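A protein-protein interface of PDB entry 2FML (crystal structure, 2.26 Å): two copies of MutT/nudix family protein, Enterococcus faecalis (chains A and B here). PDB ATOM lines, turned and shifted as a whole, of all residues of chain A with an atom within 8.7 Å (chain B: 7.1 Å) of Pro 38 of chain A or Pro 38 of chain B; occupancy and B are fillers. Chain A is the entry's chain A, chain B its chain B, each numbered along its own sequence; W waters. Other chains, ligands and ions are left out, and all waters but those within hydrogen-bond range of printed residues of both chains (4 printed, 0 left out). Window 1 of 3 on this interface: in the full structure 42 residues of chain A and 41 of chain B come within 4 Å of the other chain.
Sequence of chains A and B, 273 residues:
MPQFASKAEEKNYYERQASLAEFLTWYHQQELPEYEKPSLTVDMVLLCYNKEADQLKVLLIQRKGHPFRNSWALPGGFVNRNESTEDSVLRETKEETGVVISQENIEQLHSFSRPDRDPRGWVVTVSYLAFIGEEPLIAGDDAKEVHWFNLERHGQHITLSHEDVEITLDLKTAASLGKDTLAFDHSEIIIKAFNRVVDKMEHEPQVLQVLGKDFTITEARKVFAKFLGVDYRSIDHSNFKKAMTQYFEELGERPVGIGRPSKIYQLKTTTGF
The backbone NH of Asn 80 of chain A sits at hydrogen-bond distance from the side-chain carboxylate of Glu 83 of chain A, 3.0 Å away. The backbone NH of Ser 39 of chain A lies within hydrogen-bond range of the backbone carbonyl oxygen of Trp 122 of chain A (2.8 Å). O of Ser 39 of chain A sits at hydrogen-bond distance from N of Val 124 of chain A (2.8 Å). O of Val 124 of chain A lies within hydrogen-bond range of N of Thr 41 of chain A (2.7 Å).
Glu 36 of chain A touches Arg 81 of chain B, and with the chains exchanged Arg 81 of chain A touches Glu 36 of chain B. Lys 37 of chain A touches Ser 39 of chain B, and with the chains exchanged Ser 39 of chain A touches Lys 37 of chain B. Pro 38 of chain B touches its own counterpart, Pro 38 of chain A. Arg 81 of chain A touches Trp 122 of chain B, and with the chains exchanged Trp 122 of chain A touches Arg 81 of chain B.
Water W3 bridges the backbone carbonyl oxygen (O) of Glu 83 of chain A and the indole nitrogen (NE1) of Trp 122 of chain B. Water W4 bridges the guanidinium group of Arg 81 of chain A (3.0 Å) and the backbone carbonyl oxygen of Gly 121 of chain B (3.1 Å). Water W2 bridges N of Leu 40 of chain B (3.1 Å) and O of Glu 36 of chain A (3.2 Å).
O of Pro 115 of chain A is in hydrogen-bond range of NH2 of Arg 81 of chain B, 2.6 Å away. OH of Tyr 35 of chain A is in hydrogen-bond range of OG of Ser 39 of chain B (2.7 Å). NH2 of Arg 81 of chain A sits close to N of Trp 122 of chain B, 3.5 Å away.
Lys 37 of chain B touches Lys 37 of chain A (O to CD, 3.6 Å). CB of Lys 37 of chain A touches O of Pro 38 of chain B, 3.4 Å away. Lys 37 of chain B touches Pro 38 of chain A (CB to O, 3.4 Å). Pro 38 of chain A touches Leu 40 of chain B. Arg 81 of chain A touches Glu 36 of chain B (CG to OE1, 3.4 Å). Arg 81 of chain A touches Gly 121 of chain B. Trp 122 of chain A touches Arg 81 of chain B. Leu 40 of chain B touches Val 124 of chain A (CD2 to CG2, 3.7 Å).
Of the 13 printed residues of chain B, 10 touch a printed residue of chain A. Of the 23 printed residues of chain A, 12 touch a printed residue of chain B. Hydrophobic or aromatic side chains of chain A that line the printed part of chain B: Tyr 35, Pro 38, Leu 40, Val 79, Pro 115, Trp 122 and Val 124. Along chain A the printed residues that touch a printed residue of chain B span positions 35 to 124. Among the printed residues, no Asp or Glu carboxylate lies within 4 Å of a Lys or Arg side-chain nitrogen of the other chain.
Of the printed residues of chain B, Pro 38 of chain A touches Lys 37, Pro 38 and Leu 40. Of chain A, only Lys 37 (3.4 Å) and Pro 38 (3.5 Å) come within 4 Å of Pro 38 of chain B. Ser 39 of chain B touches just these residues of chain A: Tyr 35 (2.7 Å) and Lys 37 (3.5 Å). Of the printed residues of chain A, Lys 37 of chain B touches Lys 37, Pro 38 and Ser 39. Of the printed residues of chain A, Leu 40 of chain B touches Pro 38 (3.7 Å) and Val 124 (3.7 Å). Printed residues of chain B within 4 Å of Glu 36 of chain A: Arg 81 (3.3 Å). Of the printed residues of chain B, Arg 81 of chain A touches Glu 36 (3.4 Å), Gly 121 (3.6 Å) and Trp 122 (3.4 Å). The nearest residue of chain B that does not touch Pro 38 of chain A is Ser 39 of chain B (5.0 Å).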
ATOM      1  N   GLU A  34       5.278 -18.935  35.445  1.00  0.00           N
ATOM      2  CA  GLU A  34       6.179 -19.169  34.356  1.00  0.00           C
ATOM      3  C   GLU A  34       7.619 -18.979  34.807  1.00  0.00           C
ATOM      4  O   GLU A  34       7.929 -18.039  35.548  1.00  0.00           O
ATOM      5  CB  GLU A  34       5.851 -18.261  33.158  1.00  0.00           C
ATOM      6  CG  GLU A  34       6.688 -18.588  31.892  1.00  0.00           C
ATOM      7  CD  GLU A  34       6.456 -20.037  31.344  1.00  0.00           C
ATOM      8  OE1 GLU A  34       5.362 -20.260  30.729  1.00  0.00           O
ATOM      9  OE2 GLU A  34       7.370 -20.916  31.515  1.00  0.00           O
ATOM     10  N   TYR A  35       8.499 -19.838  34.320  1.00  0.00           N
ATOM     11  CA  TYR A  35       9.913 -19.595  34.509  1.00  0.00           C
ATOM     12  C   TYR A  35      10.691 -20.011  33.256  1.00  0.00           C
ATOM     13  O   TYR A  35      10.174 -20.693  32.392  1.00  0.00           O
ATOM     14  CB  TYR A  35      10.372 -20.255  35.802  1.00  0.00           C
ATOM     15  CG  TYR A  35       9.921 -21.664  35.865  1.00  0.00           C
ATOM     16  CD1 TYR A  35      10.685 -22.662  35.308  1.00  0.00           C
ATOM     17  CD2 TYR A  35       8.684 -22.009  36.412  1.00  0.00           C
ATOM     18  CE1 TYR A  35      10.290 -23.935  35.304  1.00  0.00           C
ATOM     19  CE2 TYR A  35       8.264 -23.291  36.397  1.00  0.00           C
ATOM     20  CZ  TYR A  35       9.113 -24.251  35.849  1.00  0.00           C
ATOM     21  OH  TYR A  35       8.763 -25.545  35.838  1.00  0.00           O
ATOM     22  N   GLU A  36      11.919 -19.550  33.143  1.00  0.00           N
ATOM     23  CA  GLU A  36      12.834 -19.951  32.070  1.00  0.00           C
ATOM     24  C   GLU A  36      13.194 -21.398  32.071  1.00  0.00           C
ATOM     25  O   GLU A  36      13.381 -22.002  33.118  1.00  0.00           O
ATOM     26  CB  GLU A  36      14.154 -19.226  32.196  1.00  0.00           C
ATOM     27  CG  GLU A  36      14.151 -17.860  31.591  1.00  0.00           C
ATOM     28  CD  GLU A  36      15.557 -17.431  31.339  1.00  0.00           C
ATOM     29  OE1 GLU A  36      16.008 -17.632  30.176  1.00  0.00           O
ATOM     30  OE2 GLU A  36      16.220 -16.989  32.328  1.00  0.00           O
ATOM     31  N   LYS A  37      13.305 -21.932  30.870  1.00  0.00           N
ATOM     32  CA  LYS A  37      13.605 -23.337  30.626  1.00  0.00           C
ATOM     33  C   LYS A  37      14.687 -23.418  29.508  1.00  0.00           C
ATOM     34  O   LYS A  37      14.794 -22.476  28.625  1.00  0.00           O
ATOM     35  CB  LYS A  37      12.311 -24.041  30.221  1.00  0.00           C
ATOM     36  CG  LYS A  37      11.221 -24.140  31.321  1.00  0.00           C
ATOM     37  CD  LYS A  37       9.800 -24.634  30.774  1.00  0.00           C
ATOM     38  CE  LYS A  37       8.691 -24.786  31.916  1.00  0.00           C
ATOM     39  NZ  LYS A  37       7.292 -25.351  31.616  1.00  0.00           N
ATOM     40  N   PRO A  38      15.533 -24.484  29.538  1.00  0.00           N
ATOM     41  CA  PRO A  38      16.449 -24.608  28.400  1.00  0.00           C
ATOM     42  C   PRO A  38      15.812 -25.311  27.199  1.00  0.00           C
ATOM     43  O   PRO A  38      14.776 -26.008  27.356  1.00  0.00           O
ATOM     44  CB  PRO A  38      17.579 -25.463  28.968  1.00  0.00           C
ATOM     45  CG  PRO A  38      16.872 -26.378  29.995  1.00  0.00           C
ATOM     46  CD  PRO A  38      15.725 -25.576  30.535  1.00  0.00           C
ATOM     47  N   SER A  39      16.413 -25.129  26.003  1.00  0.00           N
ATOM     48  CA  SER A  39      16.235 -26.088  24.913  1.00  0.00           C
ATOM     49  C   SER A  39      17.054 -27.308  25.241  1.00  0.00           C
ATOM     50  O   SER A  39      18.154 -27.246  25.861  1.00  0.00           O
ATOM     51  CB  SER A  39      16.602 -25.510  23.546  1.00  0.00           C
ATOM     52  OG  SER A  39      15.814 -24.352  23.309  1.00  0.00           O
ATOM     53  N   LEU A  40      16.499 -28.451  24.883  1.00  0.00           N
ATOM     54  CA  LEU A  40      17.116 -29.738  25.142  1.00  0.00           C
ATOM     55  C   LEU A  40      17.545 -30.374  23.823  1.00  0.00           C
ATOM     56  O   LEU A  40      16.742 -30.572  22.917  1.00  0.00           O
ATOM     57  CB  LEU A  40      16.132 -30.699  25.856  1.00  0.00           C
ATOM     58  CG  LEU A  40      16.786 -32.069  26.332  1.00  0.00           C
ATOM     59  CD1 LEU A  40      17.742 -31.692  27.446  1.00  0.00           C
ATOM     60  CD2 LEU A  40      15.715 -33.003  26.850  1.00  0.00           C
ATOM     61  N   THR A  41      18.826 -30.725  23.731  1.00  0.00           N
ATOM     62  CA  THR A  41      19.307 -31.362  22.532  1.00  0.00           C
ATOM     63  C   THR A  41      20.021 -32.650  22.910  1.00  0.00           C
ATOM     64  O   THR A  41      20.158 -32.988  24.115  1.00  0.00           O
ATOM     65  CB  THR A  41      20.308 -30.459  21.723  1.00  0.00           C
ATOM     66  OG1 THR A  41      21.394 -30.106  22.557  1.00  0.00           O
ATOM     67  CG2 THR A  41      19.696 -29.187  21.204  1.00  0.00           C
ATOM     68  N   PHE A  78      17.302 -31.176  18.413  1.00  0.00           N
ATOM     69  CA  PHE A  78      16.340 -30.852  19.456  1.00  0.00           C
ATOM     70  C   PHE A  78      15.477 -32.055  19.819  1.00  0.00           C
ATOM     71  O   PHE A  78      14.961 -32.743  18.968  1.00  0.00           O
ATOM     72  CB  PHE A  78      15.496 -29.632  19.012  1.00  0.00           C
ATOM     73  CG  PHE A  78      16.273 -28.357  19.075  1.00  0.00           C
ATOM     74  CD1 PHE A  78      16.297 -27.590  20.254  1.00  0.00           C
ATOM     75  CD2 PHE A  78      17.059 -27.942  18.003  1.00  0.00           C
ATOM     76  CE1 PHE A  78      17.086 -26.386  20.380  1.00  0.00           C
ATOM     77  CE2 PHE A  78      17.853 -26.742  18.103  1.00  0.00           C
ATOM     78  CZ  PHE A  78      17.858 -25.971  19.323  1.00  0.00           C
ATOM     79  N   VAL A  79      15.348 -32.314  21.111  1.00  0.00           N
ATOM     80  CA  VAL A  79      14.383 -33.303  21.513  1.00  0.00           C
ATOM     81  C   VAL A  79      12.975 -32.737  21.544  1.00  0.00           C
ATOM     82  O   VAL A  79      12.758 -31.645  22.063  1.00  0.00           O
ATOM     83  CB  VAL A  79      14.774 -34.205  22.748  1.00  0.00           C
ATOM     84  CG1 VAL A  79      16.292 -34.190  23.190  1.00  0.00           C
ATOM     85  CG2 VAL A  79      13.709 -34.291  23.824  1.00  0.00           C
ATOM     86  N   ASN A  80      12.034 -33.524  21.032  1.00  0.00           N
ATOM     87  CA  ASN A  80      10.620 -33.180  21.023  1.00  0.00           C
ATOM     88  C   ASN A  80       9.975 -33.598  22.362  1.00  0.00           C
ATOM     89  O   ASN A  80      10.341 -34.656  22.939  1.00  0.00           O
ATOM     90  CB  ASN A  80       9.935 -34.000  19.907  1.00  0.00           C
ATOM     91  CG  ASN A  80      10.383 -33.601  18.472  1.00  0.00           C
ATOM     92  OD1 ASN A  80      10.185 -34.390  17.544  1.00  0.00           O
ATOM     93  ND2 ASN A  80      10.900 -32.398  18.284  1.00  0.00           N
ATOM     94  N   ARG A  81       8.995 -32.801  22.820  1.00  0.00           N
ATOM     95  CA  ARG A  81       8.230 -33.090  24.061  1.00  0.00           C
ATOM     96  C   ARG A  81       7.726 -34.558  24.283  1.00  0.00           C
ATOM     97  O   ARG A  81       7.712 -35.058  25.417  1.00  0.00           O
ATOM     98  CB  ARG A  81       7.042 -32.111  24.214  1.00  0.00           C
ATOM     99  CG  ARG A  81       6.504 -32.030  25.652  1.00  0.00           C
ATOM    100  CD  ARG A  81       5.370 -32.961  25.755  1.00  0.00           C
ATOM    101  NE  ARG A  81       4.777 -33.036  27.085  1.00  0.00           N
ATOM    102  CZ  ARG A  81       5.164 -33.832  28.077  1.00  0.00           C
ATOM    103  NH1 ARG A  81       6.230 -34.660  27.981  1.00  0.00           N
ATOM    104  NH2 ARG A  81       4.464 -33.764  29.198  1.00  0.00           N
ATOM    105  N   GLU A  83       9.155 -37.422  23.355  1.00  0.00           N
ATOM    106  CA  GLU A  83      10.283 -38.306  23.059  1.00  0.00           C
ATOM    107  C   GLU A  83      11.270 -38.278  24.251  1.00  0.00           C
ATOM    108  O   GLU A  83      11.554 -37.215  24.780  1.00  0.00           O
ATOM    109  CB  GLU A  83      11.156 -37.638  21.997  1.00  0.00           C
ATOM    110  CG  GLU A  83      10.883 -37.981  20.600  1.00  0.00           C
ATOM    111  CD  GLU A  83      11.972 -37.435  19.688  1.00  0.00           C
ATOM    112  OE1 GLU A  83      12.503 -36.294  19.902  1.00  0.00           O
ATOM    113  OE2 GLU A  83      12.260 -38.177  18.730  1.00  0.00           O
ATOM    114  N   THR A  85      15.264 -38.713  25.383  1.00  0.00           N
ATOM    115  CA  THR A  85      16.489 -38.389  24.701  1.00  0.00           C
ATOM    116  C   THR A  85      17.018 -39.558  23.882  1.00  0.00           C
ATOM    117  O   THR A  85      17.581 -39.325  22.812  1.00  0.00           O
ATOM    118  CB  THR A  85      17.597 -37.826  25.630  1.00  0.00           C
ATOM    119  OG1 THR A  85      17.954 -38.788  26.631  1.00  0.00           O
ATOM    120  CG2 THR A  85      17.185 -36.478  26.263  1.00  0.00           C
ATOM    121  N   PHE A 112      25.954 -32.009  28.925  1.00  0.00           N
ATOM    122  CA  PHE A 112      26.678 -30.751  28.905  1.00  0.00           C
ATOM    123  C   PHE A 112      25.735 -29.601  29.019  1.00  0.00           C
ATOM    124  O   PHE A 112      24.742 -29.526  28.280  1.00  0.00           O
ATOM    125  CB  PHE A 112      27.438 -30.699  27.586  1.00  0.00           C
ATOM    126  CG  PHE A 112      28.529 -31.735  27.518  1.00  0.00           C
ATOM    127  CD1 PHE A 112      29.818 -31.435  27.957  1.00  0.00           C
ATOM    128  CD2 PHE A 112      28.256 -32.986  26.973  1.00  0.00           C
ATOM    129  CE1 PHE A 112      30.811 -32.418  27.901  1.00  0.00           C
ATOM    130  CE2 PHE A 112      29.227 -33.946  26.919  1.00  0.00           C
ATOM    131  CZ  PHE A 112      30.483 -33.686  27.398  1.00  0.00           C
ATOM    132  N   SER A 113      26.015 -28.744  30.002  1.00  0.00           N
ATOM    133  CA  SER A 113      25.094 -27.764  30.445  1.00  0.00           C
ATOM    134  C   SER A 113      25.729 -26.427  30.765  1.00  0.00           C
ATOM    135  O   SER A 113      25.084 -25.562  31.381  1.00  0.00           O
ATOM    136  CB  SER A 113      24.379 -28.268  31.670  1.00  0.00           C
ATOM    137  OG  SER A 113      25.317 -28.506  32.741  1.00  0.00           O
ATOM    138  N   PRO A 115      26.462 -22.817  30.799  1.00  0.00           N
ATOM    139  CA  PRO A 115      25.395 -21.862  30.469  1.00  0.00           C
ATOM    140  C   PRO A 115      25.560 -21.118  29.142  1.00  0.00           C
ATOM    141  O   PRO A 115      24.581 -20.579  28.611  1.00  0.00           O
ATOM    142  CB  PRO A 115      25.429 -20.882  31.664  1.00  0.00           C
ATOM    143  CG  PRO A 115      26.031 -21.652  32.792  1.00  0.00           C
ATOM    144  CD  PRO A 115      27.055 -22.557  32.128  1.00  0.00           C
ATOM    145  N   ARG A 117      27.382 -22.659  26.330  1.00  0.00           N
ATOM    146  CA  ARG A 117      27.840 -23.562  25.303  1.00  0.00           C
ATOM    147  C   ARG A 117      27.162 -23.355  23.899  1.00  0.00           C
ATOM    148  O   ARG A 117      27.728 -23.750  22.901  1.00  0.00           O
ATOM    149  CB  ARG A 117      27.636 -25.046  25.756  1.00  0.00           C
ATOM    150  CG  ARG A 117      26.178 -25.458  26.030  1.00  0.00           C
ATOM    151  CD  ARG A 117      26.146 -26.910  26.444  1.00  0.00           C
ATOM    152  NE  ARG A 117      26.521 -27.695  25.285  1.00  0.00           N
ATOM    153  CZ  ARG A 117      25.742 -27.887  24.221  1.00  0.00           C
ATOM    154  NH1 ARG A 117      24.499 -27.385  24.189  1.00  0.00           N
ATOM    155  NH2 ARG A 117      26.224 -28.529  23.164  1.00  0.00           N
ATOM    156  N   GLY A 121      21.157 -19.547  23.369  1.00  0.00           N
ATOM    157  CA  GLY A 121      20.784 -19.126  24.704  1.00  0.00           C
ATOM    158  C   GLY A 121      21.035 -20.299  25.589  1.00  0.00           C
ATOM    159  O   GLY A 121      22.033 -20.920  25.477  1.00  0.00           O
ATOM    160  N   TRP A 122      20.099 -20.610  26.460  1.00  0.00           N
ATOM    161  CA  TRP A 122      20.147 -21.796  27.301  1.00  0.00           C
ATOM    162  C   TRP A 122      19.776 -23.113  26.586  1.00  0.00           C
ATOM    163  O   TRP A 122      18.598 -23.419  26.327  1.00  0.00           O
ATOM    164  CB  TRP A 122      19.237 -21.558  28.484  1.00  0.00           C
ATOM    165  CG  TRP A 122      19.528 -22.480  29.738  1.00  0.00           C
ATOM    166  CD1 TRP A 122      20.590 -23.294  29.970  1.00  0.00           C
ATOM    167  CD2 TRP A 122      18.653 -22.597  30.861  1.00  0.00           C
ATOM    168  NE1 TRP A 122      20.434 -23.917  31.203  1.00  0.00           N
ATOM    169  CE2 TRP A 122      19.264 -23.479  31.774  1.00  0.00           C
ATOM    170  CE3 TRP A 122      17.374 -22.003  31.180  1.00  0.00           C
ATOM    171  CZ2 TRP A 122      18.668 -23.829  32.988  1.00  0.00           C
ATOM    172  CZ3 TRP A 122      16.808 -22.311  32.428  1.00  0.00           C
ATOM    173  CH2 TRP A 122      17.452 -23.231  33.299  1.00  0.00           C
ATOM    174  N   VAL A 123      20.812 -23.871  26.272  1.00  0.00           N
ATOM    175  CA  VAL A 123      20.680 -25.136  25.523  1.00  0.00           C
ATOM    176  C   VAL A 123      21.496 -26.202  26.224  1.00  0.00           C
ATOM    177  O   VAL A 123      22.696 -26.028  26.480  1.00  0.00           O
ATOM    178  CB  VAL A 123      21.074 -25.032  24.011  1.00  0.00           C
ATOM    179  CG1 VAL A 123      20.767 -26.357  23.258  1.00  0.00           C
ATOM    180  CG2 VAL A 123      20.345 -23.847  23.316  1.00  0.00           C
ATOM    181  N   VAL A 124      20.821 -27.310  26.577  1.00  0.00           N
ATOM    182  CA  VAL A 124      21.491 -28.424  27.291  1.00  0.00           C
ATOM    183  C   VAL A 124      21.444 -29.659  26.378  1.00  0.00           C
ATOM    184  O   VAL A 124      20.434 -29.970  25.765  1.00  0.00           O
ATOM    185  CB  VAL A 124      20.825 -28.704  28.710  1.00  0.00           C
ATOM    186  CG1 VAL A 124      21.478 -29.955  29.500  1.00  0.00           C
ATOM    187  CG2 VAL A 124      20.950 -27.460  29.556  1.00  0.00           C
ATOM    188  N   THR A 125      22.568 -30.361  26.316  1.00  0.00           N
ATOM    189  CA  THR A 125      22.650 -31.499  25.483  1.00  0.00           C
ATOM    190  C   THR A 125      22.927 -32.811  26.265  1.00  0.00           C
ATOM    191  O   THR A 125      23.671 -32.841  27.195  1.00  0.00           O
ATOM    192  CB  THR A 125      23.624 -31.201  24.345  1.00  0.00           C
ATOM    193  OG1 THR A 125      23.290 -32.002  23.213  1.00  0.00           O
ATOM    194  CG2 THR A 125      25.114 -31.477  24.743  1.00  0.00           C
ATOM    195  N   TYR B  35      10.522 -24.993  18.890  1.00  0.00           N
ATOM    196  CA  TYR B  35      10.307 -26.216  19.684  1.00  0.00           C
ATOM    197  C   TYR B  35       9.985 -25.899  21.157  1.00  0.00           C
ATOM    198  O   TYR B  35      10.641 -24.995  21.734  1.00  0.00           O
ATOM    199  CB  TYR B  35      11.581 -27.211  19.571  1.00  0.00           C
ATOM    200  N   GLU B  36       9.001 -26.624  21.753  1.00  0.00           N
ATOM    201  CA  GLU B  36       8.730 -26.676  23.261  1.00  0.00           C
ATOM    202  C   GLU B  36       9.920 -27.070  24.174  1.00  0.00           C
ATOM    203  O   GLU B  36      10.916 -27.616  23.692  1.00  0.00           O
ATOM    204  CB  GLU B  36       7.547 -27.582  23.561  1.00  0.00           C
ATOM    205  CG  GLU B  36       6.952 -27.377  24.933  1.00  0.00           C
ATOM    206  CD  GLU B  36       5.515 -27.863  25.018  1.00  0.00           C
ATOM    207  OE1 GLU B  36       5.239 -29.046  24.681  1.00  0.00           O
ATOM    208  OE2 GLU B  36       4.638 -27.034  25.394  1.00  0.00           O
ATOM    209  N   LYS B  37       9.824 -26.775  25.479  1.00  0.00           N
ATOM    210  CA  LYS B  37      10.985 -26.815  26.395  1.00  0.00           C
ATOM    211  C   LYS B  37      10.648 -27.514  27.724  1.00  0.00           C
ATOM    212  O   LYS B  37       9.565 -27.255  28.314  1.00  0.00           O
ATOM    213  CB  LYS B  37      11.498 -25.403  26.689  1.00  0.00           C
ATOM    214  CG  LYS B  37      12.182 -24.682  25.533  1.00  0.00           C
ATOM    215  CD  LYS B  37      12.379 -23.165  25.833  1.00  0.00           C
ATOM    216  CE  LYS B  37      13.493 -22.530  24.964  1.00  0.00           C
ATOM    217  NZ  LYS B  37      13.513 -21.008  24.977  1.00  0.00           N
ATOM    218  N   PRO B  38      11.538 -28.418  28.193  1.00  0.00           N
ATOM    219  CA  PRO B  38      11.226 -29.081  29.463  1.00  0.00           C
ATOM    220  C   PRO B  38      11.650 -28.205  30.647  1.00  0.00           C
ATOM    221  O   PRO B  38      12.534 -27.384  30.464  1.00  0.00           O
ATOM    222  CB  PRO B  38      12.140 -30.348  29.429  1.00  0.00           C
ATOM    223  CG  PRO B  38      13.392 -29.866  28.725  1.00  0.00           C
ATOM    224  CD  PRO B  38      12.861 -28.874  27.653  1.00  0.00           C
ATOM    225  N   SER B  39      11.088 -28.435  31.849  1.00  0.00           N
ATOM    226  CA  SER B  39      11.688 -27.953  33.092  1.00  0.00           C
ATOM    227  C   SER B  39      12.978 -28.739  33.352  1.00  0.00           C
ATOM    228  O   SER B  39      13.003 -29.968  33.185  1.00  0.00           O
ATOM    229  CB  SER B  39      10.714 -28.180  34.261  1.00  0.00           C
ATOM    230  OG  SER B  39       9.528 -27.433  34.065  1.00  0.00           O
ATOM    231  N   LEU B  40      14.048 -28.097  33.799  1.00  0.00           N
ATOM    232  CA  LEU B  40      15.313 -28.839  33.950  1.00  0.00           C
ATOM    233  C   LEU B  40      15.707 -28.963  35.441  1.00  0.00           C
ATOM    234  O   LEU B  40      15.827 -27.948  36.123  1.00  0.00           O
ATOM    235  CB  LEU B  40      16.479 -28.194  33.164  1.00  0.00           C
ATOM    236  CG  LEU B  40      17.854 -28.932  33.292  1.00  0.00           C
ATOM    237  CD1 LEU B  40      17.831 -30.312  32.625  1.00  0.00           C
ATOM    238  CD2 LEU B  40      19.079 -28.033  32.723  1.00  0.00           C
ATOM    239  N   THR B  41      15.885 -30.174  35.948  1.00  0.00           N
ATOM    240  CA  THR B  41      16.182 -30.307  37.371  1.00  0.00           C
ATOM    241  C   THR B  41      17.428 -31.154  37.554  1.00  0.00           C
ATOM    242  O   THR B  41      17.933 -31.766  36.595  1.00  0.00           O
ATOM    243  CB  THR B  41      14.970 -30.971  38.190  1.00  0.00           C
ATOM    244  OG1 THR B  41      14.704 -32.300  37.695  1.00  0.00           O
ATOM    245  CG2 THR B  41      13.666 -30.083  38.197  1.00  0.00           C
ATOM    246  N   VAL B  79      17.531 -26.350  38.020  1.00  0.00           N
ATOM    247  CA  VAL B  79      18.774 -25.687  37.526  1.00  0.00           C
ATOM    248  C   VAL B  79      18.457 -24.215  37.179  1.00  0.00           C
ATOM    249  O   VAL B  79      17.481 -23.935  36.476  1.00  0.00           O
ATOM    250  CB  VAL B  79      19.321 -26.475  36.303  1.00  0.00           C
ATOM    251  CG1 VAL B  79      20.562 -25.849  35.795  1.00  0.00           C
ATOM    252  CG2 VAL B  79      19.506 -27.978  36.721  1.00  0.00           C
ATOM    253  N   ARG B  81      19.142 -20.731  35.104  1.00  0.00           N
ATOM    254  CA  ARG B  81      19.654 -20.255  33.805  1.00  0.00           C
ATOM    255  C   ARG B  81      21.165 -19.978  33.738  1.00  0.00           C
ATOM    256  O   ARG B  81      21.827 -20.406  32.754  1.00  0.00           O
ATOM    257  CB  ARG B  81      18.752 -19.114  33.294  1.00  0.00           C
ATOM    258  CG  ARG B  81      19.282 -18.083  32.357  1.00  0.00           C
ATOM    259  CD  ARG B  81      19.213 -18.487  30.882  1.00  0.00           C
ATOM    260  NE  ARG B  81      20.410 -19.272  30.657  1.00  0.00           N
ATOM    261  CZ  ARG B  81      21.375 -18.983  29.789  1.00  0.00           C
ATOM    262  NH1 ARG B  81      21.241 -17.987  28.959  1.00  0.00           N
ATOM    263  NH2 ARG B  81      22.406 -19.796  29.711  1.00  0.00           N
ATOM    264  N   GLY B 121       3.937 -32.398  33.829  1.00  0.00           N
ATOM    265  CA  GLY B 121       4.355 -31.681  32.618  1.00  0.00           C
ATOM    266  C   GLY B 121       5.726 -32.278  32.275  1.00  0.00           C
ATOM    267  O   GLY B 121       6.206 -33.190  32.995  1.00  0.00           O
ATOM    268  N   TRP B 122       6.376 -31.729  31.246  1.00  0.00           N
ATOM    269  CA  TRP B 122       7.671 -32.163  30.723  1.00  0.00           C
ATOM    270  C   TRP B 122       8.837 -31.684  31.581  1.00  0.00           C
ATOM    271  O   TRP B 122       9.109 -30.476  31.665  1.00  0.00           O
ATOM    272  CB  TRP B 122       7.860 -31.676  29.274  1.00  0.00           C
ATOM    273  CG  TRP B 122       9.053 -32.319  28.508  1.00  0.00           C
ATOM    274  CD1 TRP B 122       9.760 -33.527  28.805  1.00  0.00           C
ATOM    275  CD2 TRP B 122       9.675 -31.764  27.344  1.00  0.00           C
ATOM    276  NE1 TRP B 122      10.746 -33.707  27.842  1.00  0.00           N
ATOM    277  CE2 TRP B 122      10.698 -32.646  26.944  1.00  0.00           C
ATOM    278  CE3 TRP B 122       9.413 -30.616  26.560  1.00  0.00           C
ATOM    279  CZ2 TRP B 122      11.491 -32.385  25.808  1.00  0.00           C
ATOM    280  CZ3 TRP B 122      10.196 -30.363  25.447  1.00  0.00           C
ATOM    281  CH2 TRP B 122      11.216 -31.249  25.084  1.00  0.00           C
ATOM    282  N   VAL B 123       9.421 -32.645  32.281  1.00  0.00           N
ATOM    283  CA  VAL B 123      10.499 -32.440  33.207  1.00  0.00           C
ATOM    284  C   VAL B 123      11.688 -33.412  32.925  1.00  0.00           C
ATOM    285  O   VAL B 123      11.553 -34.635  32.958  1.00  0.00           O
ATOM    286  CB  VAL B 123      10.090 -32.597  34.724  1.00  0.00           C
ATOM    287  CG1 VAL B 123      11.283 -32.173  35.556  1.00  0.00           C
ATOM    288  CG2 VAL B 123       8.847 -31.733  35.106  1.00  0.00           C
ATOM    289  N   VAL B 124      12.857 -32.886  32.650  1.00  0.00           N
ATOM    290  CA  VAL B 124      14.065 -33.762  32.451  1.00  0.00           C
ATOM    291  C   VAL B 124      14.986 -33.530  33.652  1.00  0.00           C
ATOM    292  O   VAL B 124      15.187 -32.371  34.116  1.00  0.00           O
ATOM    293  CB  VAL B 124      14.785 -33.376  31.083  1.00  0.00           C
ATOM    294  CG1 VAL B 124      16.170 -34.133  30.931  1.00  0.00           C
ATOM    295  CG2 VAL B 124      13.812 -33.668  29.877  1.00  0.00           C
HETATM  296  O   HOH W   1      13.558 -28.116  23.653  1.00  0.00           O
HETATM  297  O   HOH W   2      13.590 -25.052  33.942  1.00  0.00           O
HETATM  298  O   HOH W   3      12.130 -36.048  27.119  1.00  0.00           O
HETATM  299  O   HOH W   4       4.170 -35.195  31.779  1.00  0.00           O
